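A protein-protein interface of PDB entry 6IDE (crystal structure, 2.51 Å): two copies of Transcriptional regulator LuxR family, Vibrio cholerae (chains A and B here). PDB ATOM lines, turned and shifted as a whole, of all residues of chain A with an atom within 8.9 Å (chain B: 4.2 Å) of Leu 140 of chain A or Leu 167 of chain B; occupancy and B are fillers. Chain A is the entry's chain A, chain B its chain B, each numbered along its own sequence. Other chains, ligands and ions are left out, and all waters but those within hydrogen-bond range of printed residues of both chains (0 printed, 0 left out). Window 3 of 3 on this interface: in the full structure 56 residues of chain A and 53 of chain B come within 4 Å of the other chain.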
ATOM      1  N   GLY A 131      16.601 -22.513 -23.077  1.00  0.00           N
ATOM      2  CA  GLY A 131      18.056 -22.554 -23.106  1.00  0.00           C
ATOM      3  C   GLY A 131      18.689 -21.381 -22.376  1.00  0.00           C
ATOM      4  O   GLY A 131      19.659 -21.546 -21.628  1.00  0.00           O
ATOM      5  N   HIS A 132      18.147 -20.180 -22.580  1.00  0.00           N
ATOM      6  CA  HIS A 132      18.675 -19.014 -21.875  1.00  0.00           C
ATOM      7  C   HIS A 132      18.536 -19.174 -20.363  1.00  0.00           C
ATOM      8  O   HIS A 132      19.446 -18.818 -19.607  1.00  0.00           O
ATOM      9  CB  HIS A 132      17.963 -17.746 -22.355  1.00  0.00           C
ATOM     10  CG  HIS A 132      18.660 -16.480 -21.976  1.00  0.00           C
ATOM     11  ND1 HIS A 132      18.005 -15.272 -21.877  1.00  0.00           N
ATOM     12  CD2 HIS A 132      19.958 -16.233 -21.678  1.00  0.00           C
ATOM     13  CE1 HIS A 132      18.870 -14.334 -21.535  1.00  0.00           C
ATOM     14  NE2 HIS A 132      20.061 -14.890 -21.406  1.00  0.00           N
ATOM     15  N   TRP A 133      17.409 -19.723 -19.905  1.00  0.00           N
ATOM     16  CA  TRP A 133      17.188 -19.868 -18.470  1.00  0.00           C
ATOM     17  C   TRP A 133      18.118 -20.908 -17.867  1.00  0.00           C
ATOM     18  O   TRP A 133      18.589 -20.745 -16.734  1.00  0.00           O
ATOM     19  CB  TRP A 133      15.731 -20.227 -18.199  1.00  0.00           C
ATOM     20  CG  TRP A 133      14.871 -19.029 -18.030  1.00  0.00           C
ATOM     21  CD1 TRP A 133      13.877 -18.596 -18.857  1.00  0.00           C
ATOM     22  CD2 TRP A 133      14.940 -18.088 -16.957  1.00  0.00           C
ATOM     23  NE1 TRP A 133      13.316 -17.444 -18.360  1.00  0.00           N
ATOM     24  CE2 TRP A 133      13.952 -17.113 -17.194  1.00  0.00           C
ATOM     25  CE3 TRP A 133      15.739 -17.977 -15.817  1.00  0.00           C
ATOM     26  CZ2 TRP A 133      13.745 -16.041 -16.329  1.00  0.00           C
ATOM     27  CZ3 TRP A 133      15.535 -16.918 -14.971  1.00  0.00           C
ATOM     28  CH2 TRP A 133      14.546 -15.962 -15.228  1.00  0.00           C
ATOM     29  N   VAL A 134      18.395 -21.979 -18.609  1.00  0.00           N
ATOM     30  CA  VAL A 134      19.358 -22.981 -18.159  1.00  0.00           C
ATOM     31  C   VAL A 134      20.757 -22.382 -18.070  1.00  0.00           C
ATOM     32  O   VAL A 134      21.518 -22.686 -17.143  1.00  0.00           O
ATOM     33  CB  VAL A 134      19.324 -24.207 -19.089  1.00  0.00           C
ATOM     34  CG1 VAL A 134      20.475 -25.148 -18.776  1.00  0.00           C
ATOM     35  CG2 VAL A 134      17.986 -24.935 -18.961  1.00  0.00           C
ATOM     36  N   CYS A 135      21.123 -21.520 -19.020  1.00  0.00           N
ATOM     37  CA  CYS A 135      22.466 -20.944 -18.986  1.00  0.00           C
ATOM     38  C   CYS A 135      22.645 -20.033 -17.779  1.00  0.00           C
ATOM     39  O   CYS A 135      23.669 -20.104 -17.089  1.00  0.00           O
ATOM     40  CB  CYS A 135      22.760 -20.187 -20.283  1.00  0.00           C
ATOM     41  SG  CYS A 135      22.957 -21.250 -21.749  1.00  0.00           S
ATOM     42  N   ARG A 136      21.649 -19.193 -17.493  1.00  0.00           N
ATOM     43  CA  ARG A 136      21.760 -18.269 -16.368  1.00  0.00           C
ATOM     44  C   ARG A 136      21.806 -19.016 -15.040  1.00  0.00           C
ATOM     45  O   ARG A 136      22.646 -18.723 -14.183  1.00  0.00           O
ATOM     46  CB  ARG A 136      20.603 -17.274 -16.394  1.00  0.00           C
ATOM     47  CG  ARG A 136      20.602 -16.409 -17.634  1.00  0.00           C
ATOM     48  CD  ARG A 136      19.331 -15.596 -17.736  1.00  0.00           C
ATOM     49  NE  ARG A 136      19.012 -14.932 -16.478  1.00  0.00           N
ATOM     50  CZ  ARG A 136      18.100 -13.974 -16.360  1.00  0.00           C
ATOM     51  NH1 ARG A 136      17.865 -13.416 -15.175  1.00  0.00           N
ATOM     52  NH2 ARG A 136      17.431 -13.572 -17.435  1.00  0.00           N
ATOM     53  N   ALA A 137      20.924 -19.995 -14.853  1.00  0.00           N
ATOM     54  CA  ALA A 137      20.889 -20.722 -13.590  1.00  0.00           C
ATOM     55  C   ALA A 137      22.146 -21.551 -13.354  1.00  0.00           C
ATOM     56  O   ALA A 137      22.437 -21.895 -12.203  1.00  0.00           O
ATOM     57  CB  ALA A 137      19.658 -21.629 -13.536  1.00  0.00           C
ATOM     58  N   THR A 138      22.892 -21.880 -14.407  1.00  0.00           N
ATOM     59  CA  THR A 138      24.098 -22.685 -14.279  1.00  0.00           C
ATOM     60  C   THR A 138      25.374 -21.861 -14.410  1.00  0.00           C
ATOM     61  O   THR A 138      26.467 -22.434 -14.425  1.00  0.00           O
ATOM     62  CB  THR A 138      24.101 -23.810 -15.318  1.00  0.00           C
ATOM     63  OG1 THR A 138      24.033 -23.252 -16.637  1.00  0.00           O
ATOM     64  CG2 THR A 138      22.911 -24.746 -15.096  1.00  0.00           C
ATOM     65  N   GLY A 139      25.262 -20.537 -14.497  1.00  0.00           N
ATOM     66  CA  GLY A 139      26.433 -19.688 -14.625  1.00  0.00           C
ATOM     67  C   GLY A 139      27.136 -19.774 -15.962  1.00  0.00           C
ATOM     68  O   GLY A 139      28.362 -19.645 -16.018  1.00  0.00           O
ATOM     69  N   LEU A 140      26.391 -19.993 -17.045  1.00  0.00           N
ATOM     70  CA  LEU A 140      26.954 -20.068 -18.387  1.00  0.00           C
ATOM     71  C   LEU A 140      26.390 -18.972 -19.285  1.00  0.00           C
ATOM     72  O   LEU A 140      26.205 -19.173 -20.489  1.00  0.00           O
ATOM     73  CB  LEU A 140      26.719 -21.446 -19.006  1.00  0.00           C
ATOM     74  CG  LEU A 140      27.773 -22.530 -18.747  1.00  0.00           C
ATOM     75  CD1 LEU A 140      27.821 -22.947 -17.279  1.00  0.00           C
ATOM     76  CD2 LEU A 140      27.504 -23.733 -19.633  1.00  0.00           C
ATOM     77  N   SER A 141      26.111 -17.805 -18.707  1.00  0.00           N
ATOM     78  CA  SER A 141      25.626 -16.658 -19.461  1.00  0.00           C
ATOM     79  C   SER A 141      26.274 -15.411 -18.870  1.00  0.00           C
ATOM     80  O   SER A 141      27.176 -15.496 -18.029  1.00  0.00           O
ATOM     81  CB  SER A 141      24.092 -16.597 -19.433  1.00  0.00           C
ATOM     82  OG  SER A 141      23.596 -15.704 -20.415  1.00  0.00           O
ATOM     83  N   THR A 142      25.815 -14.244 -19.308  1.00  0.00           N
ATOM     84  CA  THR A 142      26.354 -12.981 -18.816  1.00  0.00           C
ATOM     85  C   THR A 142      25.250 -11.953 -18.579  1.00  0.00           C
ATOM     86  O   THR A 142      24.705 -11.379 -19.523  1.00  0.00           O
ATOM     87  CB  THR A 142      27.396 -12.401 -19.793  1.00  0.00           C
ATOM     88  OG1 THR A 142      26.947 -12.593 -21.141  1.00  0.00           O
ATOM     89  CG2 THR A 142      28.751 -13.082 -19.602  1.00  0.00           C
ATOM     90  N   TYR A 170      17.297 -18.336 -33.086  1.00  0.00           N
ATOM     91  CA  TYR A 170      17.578 -19.763 -33.187  1.00  0.00           C
ATOM     92  C   TYR A 170      19.004 -20.049 -33.635  1.00  0.00           C
ATOM     93  O   TYR A 170      19.326 -21.203 -33.935  1.00  0.00           O
ATOM     94  CB  TYR A 170      16.563 -20.445 -34.108  1.00  0.00           C
ATOM     95  CG  TYR A 170      15.213 -20.640 -33.445  1.00  0.00           C
ATOM     96  CD1 TYR A 170      14.310 -19.593 -33.367  1.00  0.00           C
ATOM     97  CD2 TYR A 170      14.845 -21.865 -32.903  1.00  0.00           C
ATOM     98  CE1 TYR A 170      13.088 -19.742 -32.764  1.00  0.00           C
ATOM     99  CE2 TYR A 170      13.603 -22.039 -32.296  1.00  0.00           C
ATOM    100  CZ  TYR A 170      12.726 -20.961 -32.225  1.00  0.00           C
ATOM    101  OH  TYR A 170      11.489 -21.073 -31.623  1.00  0.00           O
ATOM    102  N   GLY A 171      19.864 -19.032 -33.662  1.00  0.00           N
ATOM    103  CA  GLY A 171      21.277 -19.212 -33.919  1.00  0.00           C
ATOM    104  C   GLY A 171      21.682 -19.317 -35.373  1.00  0.00           C
ATOM    105  O   GLY A 171      22.802 -19.763 -35.651  1.00  0.00           O
ATOM    106  N   GLU B 163      27.812 -30.263 -22.949  1.00  0.00           N
ATOM    107  CA  GLU B 163      27.627 -28.837 -22.712  1.00  0.00           C
ATOM    108  C   GLU B 163      27.958 -28.020 -23.955  1.00  0.00           C
ATOM    109  O   GLU B 163      27.212 -27.096 -24.309  1.00  0.00           O
ATOM    110  CB  GLU B 163      28.474 -28.387 -21.528  1.00  0.00           C
ATOM    111  CG  GLU B 163      28.223 -29.210 -20.287  1.00  0.00           C
ATOM    112  CD  GLU B 163      28.915 -28.656 -19.062  1.00  0.00           C
ATOM    113  OE1 GLU B 163      28.707 -29.221 -17.969  1.00  0.00           O
ATOM    114  OE2 GLU B 163      29.662 -27.664 -19.189  1.00  0.00           O
ATOM    115  N   VAL B 164      29.055 -28.358 -24.644  1.00  0.00           N
ATOM    116  CA  VAL B 164      29.435 -27.607 -25.839  1.00  0.00           C
ATOM    117  C   VAL B 164      28.375 -27.762 -26.923  1.00  0.00           C
ATOM    118  O   VAL B 164      27.970 -26.783 -27.563  1.00  0.00           O
ATOM    119  CB  VAL B 164      30.827 -28.039 -26.338  1.00  0.00           C
ATOM    120  CG1 VAL B 164      31.119 -27.395 -27.677  1.00  0.00           C
ATOM    121  CG2 VAL B 164      31.890 -27.653 -25.333  1.00  0.00           C
ATOM    122  N   LEU B 165      27.902 -28.994 -27.142  1.00  0.00           N
ATOM    123  CA  LEU B 165      26.829 -29.197 -28.114  1.00  0.00           C
ATOM    124  C   LEU B 165      25.604 -28.371 -27.749  1.00  0.00           C
ATOM    125  O   LEU B 165      25.042 -27.665 -28.595  1.00  0.00           O
ATOM    126  CB  LEU B 165      26.465 -30.682 -28.213  1.00  0.00           C
ATOM    127  CG  LEU B 165      25.364 -31.064 -29.211  1.00  0.00           C
ATOM    128  CD1 LEU B 165      25.668 -30.536 -30.599  1.00  0.00           C
ATOM    129  CD2 LEU B 165      25.166 -32.569 -29.260  1.00  0.00           C
ATOM    130  N   PHE B 166      25.195 -28.427 -26.480  1.00  0.00           N
ATOM    131  CA  PHE B 166      24.068 -27.626 -26.014  1.00  0.00           C
ATOM    132  C   PHE B 166      24.227 -26.162 -26.417  1.00  0.00           C
ATOM    133  O   PHE B 166      23.330 -25.572 -27.031  1.00  0.00           O
ATOM    134  CB  PHE B 166      23.933 -27.785 -24.493  1.00  0.00           C
ATOM    135  CG  PHE B 166      22.834 -26.963 -23.881  1.00  0.00           C
ATOM    136  CD1 PHE B 166      21.509 -27.381 -23.960  1.00  0.00           C
ATOM    137  CD2 PHE B 166      23.127 -25.783 -23.200  1.00  0.00           C
ATOM    138  CE1 PHE B 166      20.492 -26.625 -23.386  1.00  0.00           C
ATOM    139  CE2 PHE B 166      22.120 -25.021 -22.627  1.00  0.00           C
ATOM    140  CZ  PHE B 166      20.797 -25.444 -22.715  1.00  0.00           C
ATOM    141  N   LEU B 167      25.386 -25.569 -26.121  1.00  0.00           N
ATOM    142  CA  LEU B 167      25.600 -24.161 -26.446  1.00  0.00           C
ATOM    143  C   LEU B 167      25.672 -23.921 -27.953  1.00  0.00           C
ATOM    144  O   LEU B 167      25.206 -22.877 -28.431  1.00  0.00           O
ATOM    145  CB  LEU B 167      26.865 -23.654 -25.750  1.00  0.00           C
ATOM    146  CG  LEU B 167      26.770 -23.670 -24.219  1.00  0.00           C
ATOM    147  CD1 LEU B 167      28.109 -23.398 -23.550  1.00  0.00           C
ATOM    148  CD2 LEU B 167      25.723 -22.671 -23.746  1.00  0.00           C
ATOM    149  N   LEU B 168      26.237 -24.867 -28.716  1.00  0.00           N
ATOM    150  CA  LEU B 168      26.272 -24.729 -30.171  1.00  0.00           C
ATOM    151  C   LEU B 168      24.870 -24.698 -30.771  1.00  0.00           C
ATOM    152  O   LEU B 168      24.588 -23.892 -31.665  1.00  0.00           O
ATOM    153  CB  LEU B 168      27.076 -25.870 -30.793  1.00  0.00           C
ATOM    154  CG  LEU B 168      28.579 -25.798 -30.558  1.00  0.00           C
ATOM    155  CD1 LEU B 168      29.260 -27.006 -31.159  1.00  0.00           C
ATOM    156  CD2 LEU B 168      29.128 -24.511 -31.141  1.00  0.00           C
ATOM    157  N   LEU B 169      23.980 -25.573 -30.309  1.00  0.00           N
ATOM    158  CA  LEU B 169      22.666 -25.658 -30.929  1.00  0.00           C
ATOM    159  C   LEU B 169      21.840 -24.402 -30.703  1.00  0.00           C
ATOM    160  O   LEU B 169      20.942 -24.113 -31.505  1.00  0.00           O
ATOM    161  CB  LEU B 169      21.924 -26.893 -30.413  1.00  0.00           C
ATOM    162  CG  LEU B 169      22.601 -28.219 -30.777  1.00  0.00           C
ATOM    163  CD1 LEU B 169      21.953 -29.384 -30.051  1.00  0.00           C
ATOM    164  CD2 LEU B 169      22.570 -28.441 -32.275  1.00  0.00           C
ATOM    165  N   TYR B 170      22.125 -23.649 -29.640  1.00  0.00           N
ATOM    166  CA  TYR B 170      21.469 -22.371 -29.398  1.00  0.00           C
ATOM    167  C   TYR B 170      22.191 -21.212 -30.073  1.00  0.00           C
ATOM    168  O   TYR B 170      21.821 -20.053 -29.850  1.00  0.00           O
ATOM    169  CB  TYR B 170      21.324 -22.127 -27.887  1.00  0.00           C
ATOM    170  CG  TYR B 170      20.198 -22.933 -27.274  1.00  0.00           C
ATOM    171  CD1 TYR B 170      18.900 -22.438 -27.243  1.00  0.00           C
ATOM    172  CD2 TYR B 170      20.424 -24.203 -26.754  1.00  0.00           C
ATOM    173  CE1 TYR B 170      17.859 -23.177 -26.701  1.00  0.00           C
ATOM    174  CE2 TYR B 170      19.390 -24.948 -26.208  1.00  0.00           C
ATOM    175  CZ  TYR B 170      18.110 -24.430 -26.186  1.00  0.00           C
ATOM    176  OH  TYR B 170      17.080 -25.172 -25.655  1.00  0.00           O
ATOM    177  N   GLY B 171      23.193 -21.504 -30.905  1.00  0.00           N
ATOM    178  CA  GLY B 171      23.869 -20.473 -31.674  1.00  0.00           C
ATOM    179  C   GLY B 171      24.939 -19.699 -30.935  1.00  0.00           C
ATOM    180  O   GLY B 171      25.324 -18.614 -31.383  1.00  0.00           O
ATOM    181  N   LYS B 172      25.423 -20.214 -29.808  1.00  0.00           N
ATOM    182  CA  LYS B 172      26.488 -19.553 -29.070  1.00  0.00           C
ATOM    183  C   LYS B 172      27.809 -19.695 -29.820  1.00  0.00           C
ATOM    184  O   LYS B 172      28.222 -20.804 -30.171  1.00  0.00           O
ATOM    185  CB  LYS B 172      26.592 -20.150 -27.666  1.00  0.00           C
ATOM    186  CG  LYS B 172      25.859 -19.368 -26.575  1.00  0.00           C
ATOM    187  CD  LYS B 172      24.401 -19.095 -26.910  1.00  0.00           C
ATOM    188  CE  LYS B 172      23.867 -17.928 -26.083  1.00  0.00           C
ATOM    189  NZ  LYS B 172      22.415 -17.678 -26.306  1.00  0.00           N
ATOM    190  N   HIS B 176      31.966 -16.883 -27.102  1.00  0.00           N
ATOM    191  CA  HIS B 176      31.012 -16.966 -26.002  1.00  0.00           C
ATOM    192  C   HIS B 176      31.194 -18.260 -25.213  1.00  0.00           C
ATOM    193  O   HIS B 176      31.239 -18.242 -23.976  1.00  0.00           O
ATOM    194  CB  HIS B 176      29.598 -16.846 -26.573  1.00  0.00           C
ATOM    195  CG  HIS B 176      28.519 -16.733 -25.546  1.00  0.00           C
ATOM    196  ND1 HIS B 176      28.266 -17.719 -24.618  1.00  0.00           N
ATOM    197  CD2 HIS B 176      27.594 -15.769 -25.335  1.00  0.00           C
ATOM    198  CE1 HIS B 176      27.242 -17.358 -23.865  1.00  0.00           C
ATOM    199  NE2 HIS B 176      26.814 -16.181 -24.282  1.00  0.00           N
ATOM    200  N   ILE B 177      31.328 -19.390 -25.913  1.00  0.00           N
ATOM    201  CA  ILE B 177      31.450 -20.680 -25.242  1.00  0.00           C
ATOM    202  C   ILE B 177      32.731 -20.745 -24.416  1.00  0.00           C
ATOM    203  O   ILE B 177      32.734 -21.254 -23.287  1.00  0.00           O
ATOM    204  CB  ILE B 177      31.384 -21.820 -26.273  1.00  0.00           C
ATOM    205  CG1 ILE B 177      30.058 -21.771 -27.031  1.00  0.00           C
ATOM    206  CG2 ILE B 177      31.566 -23.169 -25.599  1.00  0.00           C
ATOM    207  CD1 ILE B 177      29.811 -22.981 -27.891  1.00  0.00           C
ATOM    208  N   VAL B 180      32.257 -18.669 -21.064  1.00  0.00           N
ATOM    209  CA  VAL B 180      31.351 -19.182 -20.038  1.00  0.00           C
ATOM    210  C   VAL B 180      31.812 -20.510 -19.451  1.00  0.00           C
ATOM    211  O   VAL B 180      31.349 -20.893 -18.372  1.00  0.00           O
ATOM    212  CB  VAL B 180      29.915 -19.332 -20.579  1.00  0.00           C
ATOM    213  CG1 VAL B 180      29.351 -17.979 -20.979  1.00  0.00           C
ATOM    214  CG2 VAL B 180      29.863 -20.318 -21.749  1.00  0.00           C
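Of the 14 printed residues of chain A, 6 touch a printed residue of chain B. Printed residues of chain A that touch a printed residue of chain B: Gly 131, Val 134, Cys 135, Leu 140, Ser 141 and Gly 171. Of the 13 printed residues of chain B, 6 touch a printed residue of chain A. Hydrophobic or aromatic side chains of chain B that line the printed part of chain A: Phe 166, Leu 167, Tyr 170, His 176 and Val 180.
Gly 131 of chain A touches Tyr 170 of chain B. Val 134 of chain A touches Phe 166 of chain B. Phe 166 of chain B touches Cys 135 of chain A. Leu 167 of chain B touches Cys 135 of chain A. Leu 140 of chain A touches Leu 167 of chain B. His 176 of chain B touches Leu 140 of chain A (CE1 to O, 3.97 Å). O of Leu 140 of chain A touches CG1 of Val 180 of chain B (3.4 Å). CG1 of Val 180 of chain B touches N of Ser 141 of chain A, 3.96 Å away. CA of Gly 171 of chain B touches CA of Gly 171 of chain A (3.7 Å).
Printed residues of chain B within 4 Å of Gly 131 of chain A: Tyr 170. Leu 140 of chain A touches three residues of chain B. Of the printed residues of chain B, Gly 171 of chain A touches Gly 171 (3.7 Å). The nearest printed residue of chain B that does not touch Leu 140 of chain A is Glu 163 of chain B (4.5 Å). The nearest residue of chain A that does not touch Leu 167 of chain B is Gly 131 of chain A (6.5 Å). The nearest printed residue of chain A that does not touch Gly 171 of chain B is Tyr 170 of chain A (4.9 Å).
O of Gly 131 of chain A sits at hydrogen-bond distance from SG of Cys 135 of chain A, at 3.3 Å. O of Val 134 of chain A is in hydrogen-bond range of OG1 of Thr 138 of chain A, 2.6 Å away. The backbone carbonyl oxygen (O) of Cys 135 of chain A is in hydrogen-bond range of the side-chain hydroxyl (OG1) of Thr 138 of chain A (3.2 Å). N of Leu 140 of chain A sits at hydrogen-bond distance from O of Cys 135 of chain A, at 2.7 Å. O of Leu 167 of chain B sits at hydrogen-bond distance from N of Lys 172 of chain B.
Gly 171 of chain B touches its own counterpart, Gly 171 of chain A. Positions printed for both chains: 170 and 171.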
